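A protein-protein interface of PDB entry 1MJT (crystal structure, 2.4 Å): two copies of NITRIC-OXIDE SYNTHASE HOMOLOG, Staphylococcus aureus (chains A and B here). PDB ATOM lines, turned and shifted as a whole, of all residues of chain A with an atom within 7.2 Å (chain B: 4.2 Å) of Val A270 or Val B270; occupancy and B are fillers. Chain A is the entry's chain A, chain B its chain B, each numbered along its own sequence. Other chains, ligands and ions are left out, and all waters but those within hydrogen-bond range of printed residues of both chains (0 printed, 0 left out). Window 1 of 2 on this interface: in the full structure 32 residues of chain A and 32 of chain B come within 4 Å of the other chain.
NE of Arg A267 lies within salt-bridge range of OE2 of Glu B271 (2.8 Å). NE of Arg B267 is in salt-bridge range of OE2 of Glu A271 (2.7 Å). The side-chain hydroxyl of Ser A323 sits at hydrogen-bond distance from the side-chain carboxylate of Asp B266, 2.7 Å away.
The side-chain carboxylate (OE1) of Glu A271 is in hydrogen-bond range of a ring nitrogen (NE2) of His A187. OG of Ser A262 is in hydrogen-bond range of N of Asn A264 (3.0 Å). NH1 of Arg A267 lies within hydrogen-bond range of O of Ser A262, 2.6 Å away. NH1 of Arg A267 sits close to O of Phe A263 (3.5 Å). The guanidinium group (NH1) of Arg A267 sits at hydrogen-bond distance from the side-chain amide oxygen (OD1) of Asn A264, 2.9 Å away. ND2 of Asn A273 is in hydrogen-bond range of O of Leu A269.
O of Phe A263 touches CG1 of Val B270, 3.8 Å away. Phe A263 touches Asn B273. CD2 of Tyr B274 touches CD1 of Phe A263 (3.8 Å). Arg A267 touches Val B270. Arg A267 touches Tyr B274 (NH2 to CD2, 3.4 Å). Phe B263 touches Val A270. Val A270 touches Asp B266. Arg B267 touches Val A270 (CG to CG1, 3.7 Å). Phe B263 touches Asn A273 (CZ to O, 3.7 Å). Tyr A274 touches Phe B263.
Printed residues of chain A within 4 Å of Val B270: Phe A263 (3.8 Å), Asp A266 (3.6 Å), Arg A267 (3.9 Å) and Val A270 (3.9 Å). Of the printed residues of chain A, Arg B267 touches Val A270 (3.7 Å), Glu A271 (2.7 Å) and Tyr A274 (3.4 Å). Printed residues of chain B within 4 Å of Ser A262: Tyr B274. Of the printed residues of chain B, Arg A267 touches Val B270, Glu B271 and Tyr B274. Val A276 touches none of the printed residues of chain B. The nearest printed residue of chain A that does not touch Phe B263 is Leu A322 (4.7 Å).
Of the 10 printed residues of chain B, 8 touch a printed residue of chain A. Printed residues of chain B that touch a printed residue of chain A: Phe B263, Asp B266, Arg B267, Leu B269, Val B270, Glu B271, Asn B273 and Tyr B274. Hydrophobic or aromatic side chains of chain B within 4 Å of the printed part of chain A: Phe B263, Leu B269, Val B270 and Tyr B274. Printed residues of chain A that touch a printed residue of chain B: Ser A262, Phe A263, Asp A266, Arg A267, Val A270, Glu A271, Asn A273, Tyr A274 and Ser A323. Hydrophobic or aromatic side chains of chain A within 4 Å of the printed part of chain B: Phe A263, Val A270 and Tyr A274. Among the printed residues, Asp or Glu carboxylates within 4 Å of a Lys or Arg side-chain nitrogen of the other chain: Arg A267 with Glu B271 (2.8 Å) and Glu A271 with Arg B267 (2.7 Å).
Phe A263 touches Val B270, and with the chains exchanged Val A270 touches Phe B263. Phe A263 touches Asn B273, and with the chains exchanged Asn A273 touches Phe B263. Arg A267 touches Val B270, and with the chains exchanged Val A270 touches Arg B267. Val B270 touches its own counterpart, Val A270. 10 positions are printed for both chains.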
ATOM      1  N   HIS A 187      -2.969 -29.083 -27.125  1.00  0.00           N
ATOM      2  CA  HIS A 187      -3.434 -28.661 -25.813  1.00  0.00           C
ATOM      3  C   HIS A 187      -2.260 -28.761 -24.843  1.00  0.00           C
ATOM      4  O   HIS A 187      -1.746 -29.852 -24.567  1.00  0.00           O
ATOM      5  CB  HIS A 187      -4.572 -29.559 -25.339  1.00  0.00           C
ATOM      6  CG  HIS A 187      -5.388 -28.962 -24.238  1.00  0.00           C
ATOM      7  ND1 HIS A 187      -4.822 -28.393 -23.116  1.00  0.00           N
ATOM      8  CD2 HIS A 187      -6.729 -28.841 -24.087  1.00  0.00           C
ATOM      9  CE1 HIS A 187      -5.779 -27.946 -22.324  1.00  0.00           C
ATOM     10  NE2 HIS A 187      -6.946 -28.205 -22.890  1.00  0.00           N
ATOM     11  N   GLY A 233     -13.774 -25.341 -33.131  1.00  0.00           N
ATOM     12  CA  GLY A 233     -13.847 -26.239 -31.984  1.00  0.00           C
ATOM     13  C   GLY A 233     -15.141 -26.961 -31.665  1.00  0.00           C
ATOM     14  O   GLY A 233     -15.117 -27.990 -30.982  1.00  0.00           O
ATOM     15  N   VAL A 234     -16.267 -26.442 -32.145  1.00  0.00           N
ATOM     16  CA  VAL A 234     -17.558 -27.074 -31.882  1.00  0.00           C
ATOM     17  C   VAL A 234     -18.202 -27.660 -33.144  1.00  0.00           C
ATOM     18  O   VAL A 234     -18.503 -28.846 -33.218  1.00  0.00           O
ATOM     19  CB  VAL A 234     -18.563 -26.060 -31.239  1.00  0.00           C
ATOM     20  CG1 VAL A 234     -19.877 -26.755 -30.917  1.00  0.00           C
ATOM     21  CG2 VAL A 234     -17.977 -25.465 -29.968  1.00  0.00           C
ATOM     22  N   PHE A 253      -8.106 -36.387 -23.835  1.00  0.00           N
ATOM     23  CA  PHE A 253      -8.289 -35.655 -22.585  1.00  0.00           C
ATOM     24  C   PHE A 253      -8.424 -36.625 -21.426  1.00  0.00           C
ATOM     25  O   PHE A 253      -8.645 -36.227 -20.283  1.00  0.00           O
ATOM     26  CB  PHE A 253      -9.522 -34.754 -22.676  1.00  0.00           C
ATOM     27  CG  PHE A 253      -9.416 -33.690 -23.730  1.00  0.00           C
ATOM     28  CD1 PHE A 253     -10.560 -33.138 -24.298  1.00  0.00           C
ATOM     29  CD2 PHE A 253      -8.170 -33.248 -24.170  1.00  0.00           C
ATOM     30  CE1 PHE A 253     -10.462 -32.167 -25.291  1.00  0.00           C
ATOM     31  CE2 PHE A 253      -8.061 -32.278 -25.162  1.00  0.00           C
ATOM     32  CZ  PHE A 253      -9.210 -31.737 -25.725  1.00  0.00           C
ATOM     33  N   SER A 262     -21.871 -37.992 -16.785  1.00  0.00           N
ATOM     34  CA  SER A 262     -20.514 -37.566 -16.440  1.00  0.00           C
ATOM     35  C   SER A 262     -20.239 -36.110 -16.754  1.00  0.00           C
ATOM     36  O   SER A 262     -19.407 -35.475 -16.106  1.00  0.00           O
ATOM     37  CB  SER A 262     -19.494 -38.414 -17.201  1.00  0.00           C
ATOM     38  OG  SER A 262     -19.449 -38.028 -18.568  1.00  0.00           O
ATOM     39  N   PHE A 263     -20.937 -35.593 -17.759  1.00  0.00           N
ATOM     40  CA  PHE A 263     -20.759 -34.219 -18.214  1.00  0.00           C
ATOM     41  C   PHE A 263     -19.383 -34.090 -18.858  1.00  0.00           C
ATOM     42  O   PHE A 263     -18.879 -32.989 -19.049  1.00  0.00           O
ATOM     43  CB  PHE A 263     -20.904 -33.218 -17.057  1.00  0.00           C
ATOM     44  CG  PHE A 263     -22.326 -33.024 -16.593  1.00  0.00           C
ATOM     45  CD1 PHE A 263     -22.920 -33.929 -15.718  1.00  0.00           C
ATOM     46  CD2 PHE A 263     -23.084 -31.957 -17.064  1.00  0.00           C
ATOM     47  CE1 PHE A 263     -24.254 -33.783 -15.320  1.00  0.00           C
ATOM     48  CE2 PHE A 263     -24.415 -31.796 -16.676  1.00  0.00           C
ATOM     49  CZ  PHE A 263     -25.004 -32.715 -15.800  1.00  0.00           C
ATOM     50  N   ASN A 264     -18.775 -35.223 -19.193  1.00  0.00           N
ATOM     51  CA  ASN A 264     -17.469 -35.204 -19.838  1.00  0.00           C
ATOM     52  C   ASN A 264     -17.608 -34.719 -21.274  1.00  0.00           C
ATOM     53  O   ASN A 264     -16.710 -34.063 -21.802  1.00  0.00           O
ATOM     54  CB  ASN A 264     -16.822 -36.590 -19.825  1.00  0.00           C
ATOM     55  CG  ASN A 264     -16.112 -36.884 -18.522  1.00  0.00           C
ATOM     56  OD1 ASN A 264     -15.636 -35.974 -17.845  1.00  0.00           O
ATOM     57  ND2 ASN A 264     -16.022 -38.164 -18.171  1.00  0.00           N
ATOM     58  N   LYS A 265     -18.727 -35.054 -21.912  1.00  0.00           N
ATOM     59  CA  LYS A 265     -18.957 -34.595 -23.275  1.00  0.00           C
ATOM     60  C   LYS A 265     -18.861 -33.073 -23.247  1.00  0.00           C
ATOM     61  O   LYS A 265     -18.271 -32.458 -24.133  1.00  0.00           O
ATOM     62  CB  LYS A 265     -20.343 -35.008 -23.772  1.00  0.00           C
ATOM     63  CG  LYS A 265     -20.462 -36.451 -24.201  1.00  0.00           C
ATOM     64  CD  LYS A 265     -21.795 -36.664 -24.887  1.00  0.00           C
ATOM     65  CE  LYS A 265     -22.046 -38.128 -25.173  1.00  0.00           C
ATOM     66  NZ  LYS A 265     -23.410 -38.346 -25.743  1.00  0.00           N
ATOM     67  N   ASP A 266     -19.435 -32.475 -22.206  1.00  0.00           N
ATOM     68  CA  ASP A 266     -19.410 -31.027 -22.048  1.00  0.00           C
ATOM     69  C   ASP A 266     -18.006 -30.502 -21.773  1.00  0.00           C
ATOM     70  O   ASP A 266     -17.631 -29.456 -22.295  1.00  0.00           O
ATOM     71  CB  ASP A 266     -20.354 -30.604 -20.918  1.00  0.00           C
ATOM     72  CG  ASP A 266     -21.745 -31.176 -21.084  1.00  0.00           C
ATOM     73  OD1 ASP A 266     -21.997 -32.299 -20.597  1.00  0.00           O
ATOM     74  OD2 ASP A 266     -22.584 -30.509 -21.722  1.00  0.00           O
ATOM     75  N   ARG A 267     -17.230 -31.222 -20.959  1.00  0.00           N
ATOM     76  CA  ARG A 267     -15.857 -30.811 -20.630  1.00  0.00           C
ATOM     77  C   ARG A 267     -14.954 -30.887 -21.855  1.00  0.00           C
ATOM     78  O   ARG A 267     -14.126 -30.001 -22.098  1.00  0.00           O
ATOM     79  CB  ARG A 267     -15.270 -31.694 -19.531  1.00  0.00           C
ATOM     80  CG  ARG A 267     -15.928 -31.538 -18.175  1.00  0.00           C
ATOM     81  CD  ARG A 267     -15.144 -32.291 -17.103  1.00  0.00           C
ATOM     82  NE  ARG A 267     -15.820 -32.232 -15.810  1.00  0.00           N
ATOM     83  CZ  ARG A 267     -16.769 -33.074 -15.410  1.00  0.00           C
ATOM     84  NH1 ARG A 267     -17.165 -34.068 -16.195  1.00  0.00           N
ATOM     85  NH2 ARG A 267     -17.342 -32.900 -14.230  1.00  0.00           N
ATOM     86  N   ALA A 268     -15.121 -31.958 -22.624  1.00  0.00           N
ATOM     87  CA  ALA A 268     -14.340 -32.166 -23.838  1.00  0.00           C
ATOM     88  C   ALA A 268     -14.501 -30.975 -24.786  1.00  0.00           C
ATOM     89  O   ALA A 268     -13.524 -30.500 -25.378  1.00  0.00           O
ATOM     90  CB  ALA A 268     -14.785 -33.460 -24.527  1.00  0.00           C
ATOM     91  N   LEU A 269     -15.736 -30.494 -24.920  1.00  0.00           N
ATOM     92  CA  LEU A 269     -16.021 -29.361 -25.793  1.00  0.00           C
ATOM     93  C   LEU A 269     -15.258 -28.118 -25.327  1.00  0.00           C
ATOM     94  O   LEU A 269     -14.599 -27.446 -26.127  1.00  0.00           O
ATOM     95  CB  LEU A 269     -17.530 -29.085 -25.813  1.00  0.00           C
ATOM     96  CG  LEU A 269     -18.180 -28.850 -27.179  1.00  0.00           C
ATOM     97  CD1 LEU A 269     -17.822 -29.994 -28.117  1.00  0.00           C
ATOM     98  CD2 LEU A 269     -19.694 -28.743 -27.019  1.00  0.00           C
ATOM     99  N   VAL A 270     -15.341 -27.818 -24.034  1.00  0.00           N
ATOM    100  CA  VAL A 270     -14.644 -26.655 -23.490  1.00  0.00           C
ATOM    101  C   VAL A 270     -13.135 -26.801 -23.737  1.00  0.00           C
ATOM    102  O   VAL A 270     -12.493 -25.893 -24.275  1.00  0.00           O
ATOM    103  CB  VAL A 270     -14.907 -26.485 -21.956  1.00  0.00           C
ATOM    104  CG1 VAL A 270     -14.122 -25.286 -21.410  1.00  0.00           C
ATOM    105  CG2 VAL A 270     -16.390 -26.280 -21.696  1.00  0.00           C
ATOM    106  N   GLU A 271     -12.575 -27.948 -23.362  1.00  0.00           N
ATOM    107  CA  GLU A 271     -11.151 -28.168 -23.563  1.00  0.00           C
ATOM    108  C   GLU A 271     -10.721 -28.045 -25.029  1.00  0.00           C
ATOM    109  O   GLU A 271      -9.704 -27.413 -25.330  1.00  0.00           O
ATOM    110  CB  GLU A 271     -10.739 -29.540 -23.021  1.00  0.00           C
ATOM    111  CG  GLU A 271     -10.878 -29.700 -21.507  1.00  0.00           C
ATOM    112  CD  GLU A 271     -10.255 -28.547 -20.713  1.00  0.00           C
ATOM    113  OE1 GLU A 271      -9.222 -27.993 -21.152  1.00  0.00           O
ATOM    114  OE2 GLU A 271     -10.801 -28.206 -19.637  1.00  0.00           O
ATOM    115  N   LEU A 272     -11.490 -28.640 -25.940  1.00  0.00           N
ATOM    116  CA  LEU A 272     -11.147 -28.575 -27.357  1.00  0.00           C
ATOM    117  C   LEU A 272     -11.088 -27.139 -27.873  1.00  0.00           C
ATOM    118  O   LEU A 272     -10.218 -26.794 -28.672  1.00  0.00           O
ATOM    119  CB  LEU A 272     -12.135 -29.382 -28.201  1.00  0.00           C
ATOM    120  CG  LEU A 272     -11.731 -29.457 -29.684  1.00  0.00           C
ATOM    121  CD1 LEU A 272     -10.337 -30.079 -29.816  1.00  0.00           C
ATOM    122  CD2 LEU A 272     -12.753 -30.270 -30.465  1.00  0.00           C
ATOM    123  N   ASN A 273     -12.011 -26.301 -27.421  1.00  0.00           N
ATOM    124  CA  ASN A 273     -12.019 -24.903 -27.846  1.00  0.00           C
ATOM    125  C   ASN A 273     -10.879 -24.141 -27.188  1.00  0.00           C
ATOM    126  O   ASN A 273     -10.388 -23.146 -27.726  1.00  0.00           O
ATOM    127  CB  ASN A 273     -13.364 -24.256 -27.507  1.00  0.00           C
ATOM    128  CG  ASN A 273     -14.433 -24.595 -28.526  1.00  0.00           C
ATOM    129  OD1 ASN A 273     -14.595 -23.901 -29.526  1.00  0.00           O
ATOM    130  ND2 ASN A 273     -15.151 -25.687 -28.291  1.00  0.00           N
ATOM    131  N   TYR A 274     -10.460 -24.610 -26.020  1.00  0.00           N
ATOM    132  CA  TYR A 274      -9.356 -23.974 -25.322  1.00  0.00           C
ATOM    133  C   TYR A 274      -8.081 -24.263 -26.103  1.00  0.00           C
ATOM    134  O   TYR A 274      -7.212 -23.407 -26.230  1.00  0.00           O
ATOM    135  CB  TYR A 274      -9.245 -24.516 -23.900  1.00  0.00           C
ATOM    136  CG  TYR A 274      -7.983 -24.092 -23.178  1.00  0.00           C
ATOM    137  CD1 TYR A 274      -6.799 -24.824 -23.311  1.00  0.00           C
ATOM    138  CD2 TYR A 274      -7.967 -22.955 -22.371  1.00  0.00           C
ATOM    139  CE1 TYR A 274      -5.629 -24.434 -22.656  1.00  0.00           C
ATOM    140  CE2 TYR A 274      -6.799 -22.557 -21.711  1.00  0.00           C
ATOM    141  CZ  TYR A 274      -5.638 -23.300 -21.861  1.00  0.00           C
ATOM    142  OH  TYR A 274      -4.482 -22.896 -21.235  1.00  0.00           O
ATOM    143  N   ALA A 275      -7.988 -25.479 -26.630  1.00  0.00           N
ATOM    144  CA  ALA A 275      -6.833 -25.896 -27.412  1.00  0.00           C
ATOM    145  C   ALA A 275      -6.803 -25.139 -28.737  1.00  0.00           C
ATOM    146  O   ALA A 275      -5.777 -24.588 -29.129  1.00  0.00           O
ATOM    147  CB  ALA A 275      -6.898 -27.401 -27.671  1.00  0.00           C
ATOM    148  N   VAL A 276      -7.932 -25.117 -29.432  1.00  0.00           N
ATOM    149  CA  VAL A 276      -8.007 -24.425 -30.711  1.00  0.00           C
ATOM    150  C   VAL A 276      -7.559 -22.982 -30.549  1.00  0.00           C
ATOM    151  O   VAL A 276      -6.657 -22.525 -31.253  1.00  0.00           O
ATOM    152  CB  VAL A 276      -9.456 -24.436 -31.291  1.00  0.00           C
ATOM    153  CG1 VAL A 276      -9.550 -23.484 -32.486  1.00  0.00           C
ATOM    154  CG2 VAL A 276      -9.854 -25.857 -31.708  1.00  0.00           C
ATOM    155  N   LEU A 322     -21.589 -22.407 -27.283  1.00  0.00           N
ATOM    156  CA  LEU A 322     -20.819 -22.680 -26.084  1.00  0.00           C
ATOM    157  C   LEU A 322     -21.136 -21.614 -25.042  1.00  0.00           C
ATOM    158  O   LEU A 322     -20.921 -20.427 -25.282  1.00  0.00           O
ATOM    159  CB  LEU A 322     -19.323 -22.667 -26.395  1.00  0.00           C
ATOM    160  CG  LEU A 322     -18.458 -23.435 -25.392  1.00  0.00           C
ATOM    161  CD1 LEU A 322     -18.716 -24.930 -25.556  1.00  0.00           C
ATOM    162  CD2 LEU A 322     -16.996 -23.132 -25.621  1.00  0.00           C
ATOM    163  N   SER A 323     -21.658 -22.040 -23.892  1.00  0.00           N
ATOM    164  CA  SER A 323     -21.999 -21.116 -22.816  1.00  0.00           C
ATOM    165  C   SER A 323     -22.740 -19.904 -23.380  1.00  0.00           C
ATOM    166  O   SER A 323     -22.401 -18.757 -23.096  1.00  0.00           O
ATOM    167  CB  SER A 323     -20.723 -20.667 -22.098  1.00  0.00           C
ATOM    168  OG  SER A 323     -20.079 -21.762 -21.464  1.00  0.00           O
ATOM    169  N   PHE B 263     -11.187 -19.622 -20.580  1.00  0.00           N
ATOM    170  CA  PHE B 263     -12.296 -20.575 -20.681  1.00  0.00           C
ATOM    171  C   PHE B 263     -12.766 -21.129 -19.342  1.00  0.00           C
ATOM    172  O   PHE B 263     -13.553 -22.083 -19.292  1.00  0.00           O
ATOM    173  CB  PHE B 263     -11.938 -21.727 -21.632  1.00  0.00           C
ATOM    174  CG  PHE B 263     -11.827 -21.305 -23.072  1.00  0.00           C
ATOM    175  CD1 PHE B 263     -10.692 -20.639 -23.534  1.00  0.00           C
ATOM    176  CD2 PHE B 263     -12.891 -21.496 -23.948  1.00  0.00           C
ATOM    177  CE1 PHE B 263     -10.621 -20.161 -24.845  1.00  0.00           C
ATOM    178  CE2 PHE B 263     -12.835 -21.024 -25.255  1.00  0.00           C
ATOM    179  CZ  PHE B 263     -11.697 -20.352 -25.709  1.00  0.00           C
ATOM    180  N   ASP B 266     -16.508 -21.099 -18.700  1.00  0.00           N
ATOM    181  CA  ASP B 266     -17.180 -22.246 -19.298  1.00  0.00           C
ATOM    182  C   ASP B 266     -16.963 -23.519 -18.483  1.00  0.00           C
ATOM    183  O   ASP B 266     -17.851 -24.359 -18.388  1.00  0.00           O
ATOM    184  CB  ASP B 266     -16.673 -22.469 -20.729  1.00  0.00           C
ATOM    185  CG  ASP B 266     -16.662 -21.190 -21.568  1.00  0.00           C
ATOM    186  OD1 ASP B 266     -15.664 -20.430 -21.528  1.00  0.00           O
ATOM    187  OD2 ASP B 266     -17.662 -20.949 -22.272  1.00  0.00           O
ATOM    188  N   ARG B 267     -15.774 -23.679 -17.914  1.00  0.00           N
ATOM    189  CA  ARG B 267     -15.504 -24.861 -17.104  1.00  0.00           C
ATOM    190  C   ARG B 267     -16.324 -24.739 -15.836  1.00  0.00           C
ATOM    191  O   ARG B 267     -16.849 -25.722 -15.324  1.00  0.00           O
ATOM    192  CB  ARG B 267     -14.025 -24.957 -16.723  1.00  0.00           C
ATOM    193  CG  ARG B 267     -13.075 -25.212 -17.881  1.00  0.00           C
ATOM    194  CD  ARG B 267     -11.655 -25.500 -17.379  1.00  0.00           C
ATOM    195  NE  ARG B 267     -10.749 -25.774 -18.487  1.00  0.00           N
ATOM    196  CZ  ARG B 267     -10.083 -24.838 -19.150  1.00  0.00           C
ATOM    197  NH1 ARG B 267     -10.216 -23.568 -18.797  1.00  0.00           N
ATOM    198  NH2 ARG B 267      -9.316 -25.165 -20.181  1.00  0.00           N
ATOM    199  N   ALA B 268     -16.428 -23.516 -15.333  1.00  0.00           N
ATOM    200  CA  ALA B 268     -17.173 -23.262 -14.118  1.00  0.00           C
ATOM    201  C   ALA B 268     -18.619 -23.676 -14.324  1.00  0.00           C
ATOM    202  O   ALA B 268     -19.215 -24.319 -13.458  1.00  0.00           O
ATOM    203  CB  ALA B 268     -17.083 -21.791 -13.753  1.00  0.00           C
ATOM    204  N   LEU B 269     -19.173 -23.326 -15.482  1.00  0.00           N
ATOM    205  CA  LEU B 269     -20.560 -23.656 -15.822  1.00  0.00           C
ATOM    206  C   LEU B 269     -20.804 -25.172 -15.888  1.00  0.00           C
ATOM    207  O   LEU B 269     -21.800 -25.681 -15.363  1.00  0.00           O
ATOM    208  CB  LEU B 269     -20.930 -23.022 -17.172  1.00  0.00           C
ATOM    209  CG  LEU B 269     -22.345 -22.472 -17.326  1.00  0.00           C
ATOM    210  CD1 LEU B 269     -22.506 -21.265 -16.433  1.00  0.00           C
ATOM    211  CD2 LEU B 269     -22.596 -22.076 -18.768  1.00  0.00           C
ATOM    212  N   VAL B 270     -19.895 -25.891 -16.535  1.00  0.00           N
ATOM    213  CA  VAL B 270     -20.036 -27.331 -16.667  1.00  0.00           C
ATOM    214  C   VAL B 270     -19.939 -28.007 -15.308  1.00  0.00           C
ATOM    215  O   VAL B 270     -20.682 -28.950 -15.016  1.00  0.00           O
ATOM    216  CB  VAL B 270     -18.944 -27.926 -17.598  1.00  0.00           C
ATOM    217  CG1 VAL B 270     -19.177 -29.405 -17.784  1.00  0.00           C
ATOM    218  CG2 VAL B 270     -18.959 -27.228 -18.947  1.00  0.00           C
ATOM    219  N   GLU B 271     -19.017 -27.519 -14.483  1.00  0.00           N
ATOM    220  CA  GLU B 271     -18.800 -28.078 -13.152  1.00  0.00           C
ATOM    221  C   GLU B 271     -19.982 -27.857 -12.208  1.00  0.00           C
ATOM    222  O   GLU B 271     -20.344 -28.742 -11.426  1.00  0.00           O
ATOM    223  CB  GLU B 271     -17.521 -27.492 -12.534  1.00  0.00           C
ATOM    224  CG  GLU B 271     -16.208 -27.970 -13.192  1.00  0.00           C
ATOM    225  CD  GLU B 271     -16.095 -29.500 -13.303  1.00  0.00           C
ATOM    226  OE1 GLU B 271     -16.666 -30.215 -12.451  1.00  0.00           O
ATOM    227  OE2 GLU B 271     -15.423 -29.991 -14.235  1.00  0.00           O
ATOM    228  N   LEU B 272     -20.589 -26.681 -12.288  1.00  0.00           N
ATOM    229  CA  LEU B 272     -21.732 -26.366 -11.440  1.00  0.00           C
ATOM    230  C   LEU B 272     -22.951 -27.243 -11.767  1.00  0.00           C
ATOM    231  O   LEU B 272     -23.736 -27.587 -10.883  1.00  0.00           O
ATOM    232  CB  LEU B 272     -22.092 -24.885 -11.589  1.00  0.00           C
ATOM    233  CG  LEU B 272     -23.322 -24.370 -10.838  1.00  0.00           C
ATOM    234  CD1 LEU B 272     -23.266 -24.750  -9.365  1.00  0.00           C
ATOM    235  CD2 LEU B 272     -23.389 -22.870 -11.003  1.00  0.00           C
ATOM    236  N   ASN B 273     -23.105 -27.603 -13.039  1.00  0.00           N
ATOM    237  CA  ASN B 273     -24.222 -28.442 -13.465  1.00  0.00           C
ATOM    238  C   ASN B 273     -23.944 -29.877 -13.081  1.00  0.00           C
ATOM    239  O   ASN B 273     -24.867 -30.638 -12.798  1.00  0.00           O
ATOM    240  CB  ASN B 273     -24.437 -28.323 -14.977  1.00  0.00           C
ATOM    241  CG  ASN B 273     -25.302 -27.135 -15.346  1.00  0.00           C
ATOM    242  OD1 ASN B 273     -26.528 -27.195 -15.248  1.00  0.00           O
ATOM    243  ND2 ASN B 273     -24.665 -26.041 -15.751  1.00  0.00           N
ATOM    244  N   TYR B 274     -22.668 -30.248 -13.080  1.00  0.00           N
ATOM    245  CA  TYR B 274     -22.282 -31.589 -12.672  1.00  0.00           C
ATOM    246  C   TYR B 274     -22.677 -31.735 -11.204  1.00  0.00           C
ATOM    247  O   TYR B 274     -23.229 -32.757 -10.781  1.00  0.00           O
ATOM    248  CB  TYR B 274     -20.773 -31.780 -12.827  1.00  0.00           C
ATOM    249  CG  TYR B 274     -20.272 -33.081 -12.242  1.00  0.00           C
ATOM    250  CD1 TYR B 274     -19.878 -33.166 -10.901  1.00  0.00           C
ATOM    251  CD2 TYR B 274     -20.213 -34.239 -13.013  1.00  0.00           C
ATOM    252  CE1 TYR B 274     -19.441 -34.378 -10.338  1.00  0.00           C
ATOM    253  CE2 TYR B 274     -19.775 -35.457 -12.461  1.00  0.00           C
ATOM    254  CZ  TYR B 274     -19.392 -35.518 -11.124  1.00  0.00           C
ATOM    255  OH  TYR B 274     -18.973 -36.717 -10.581  1.00  0.00           O
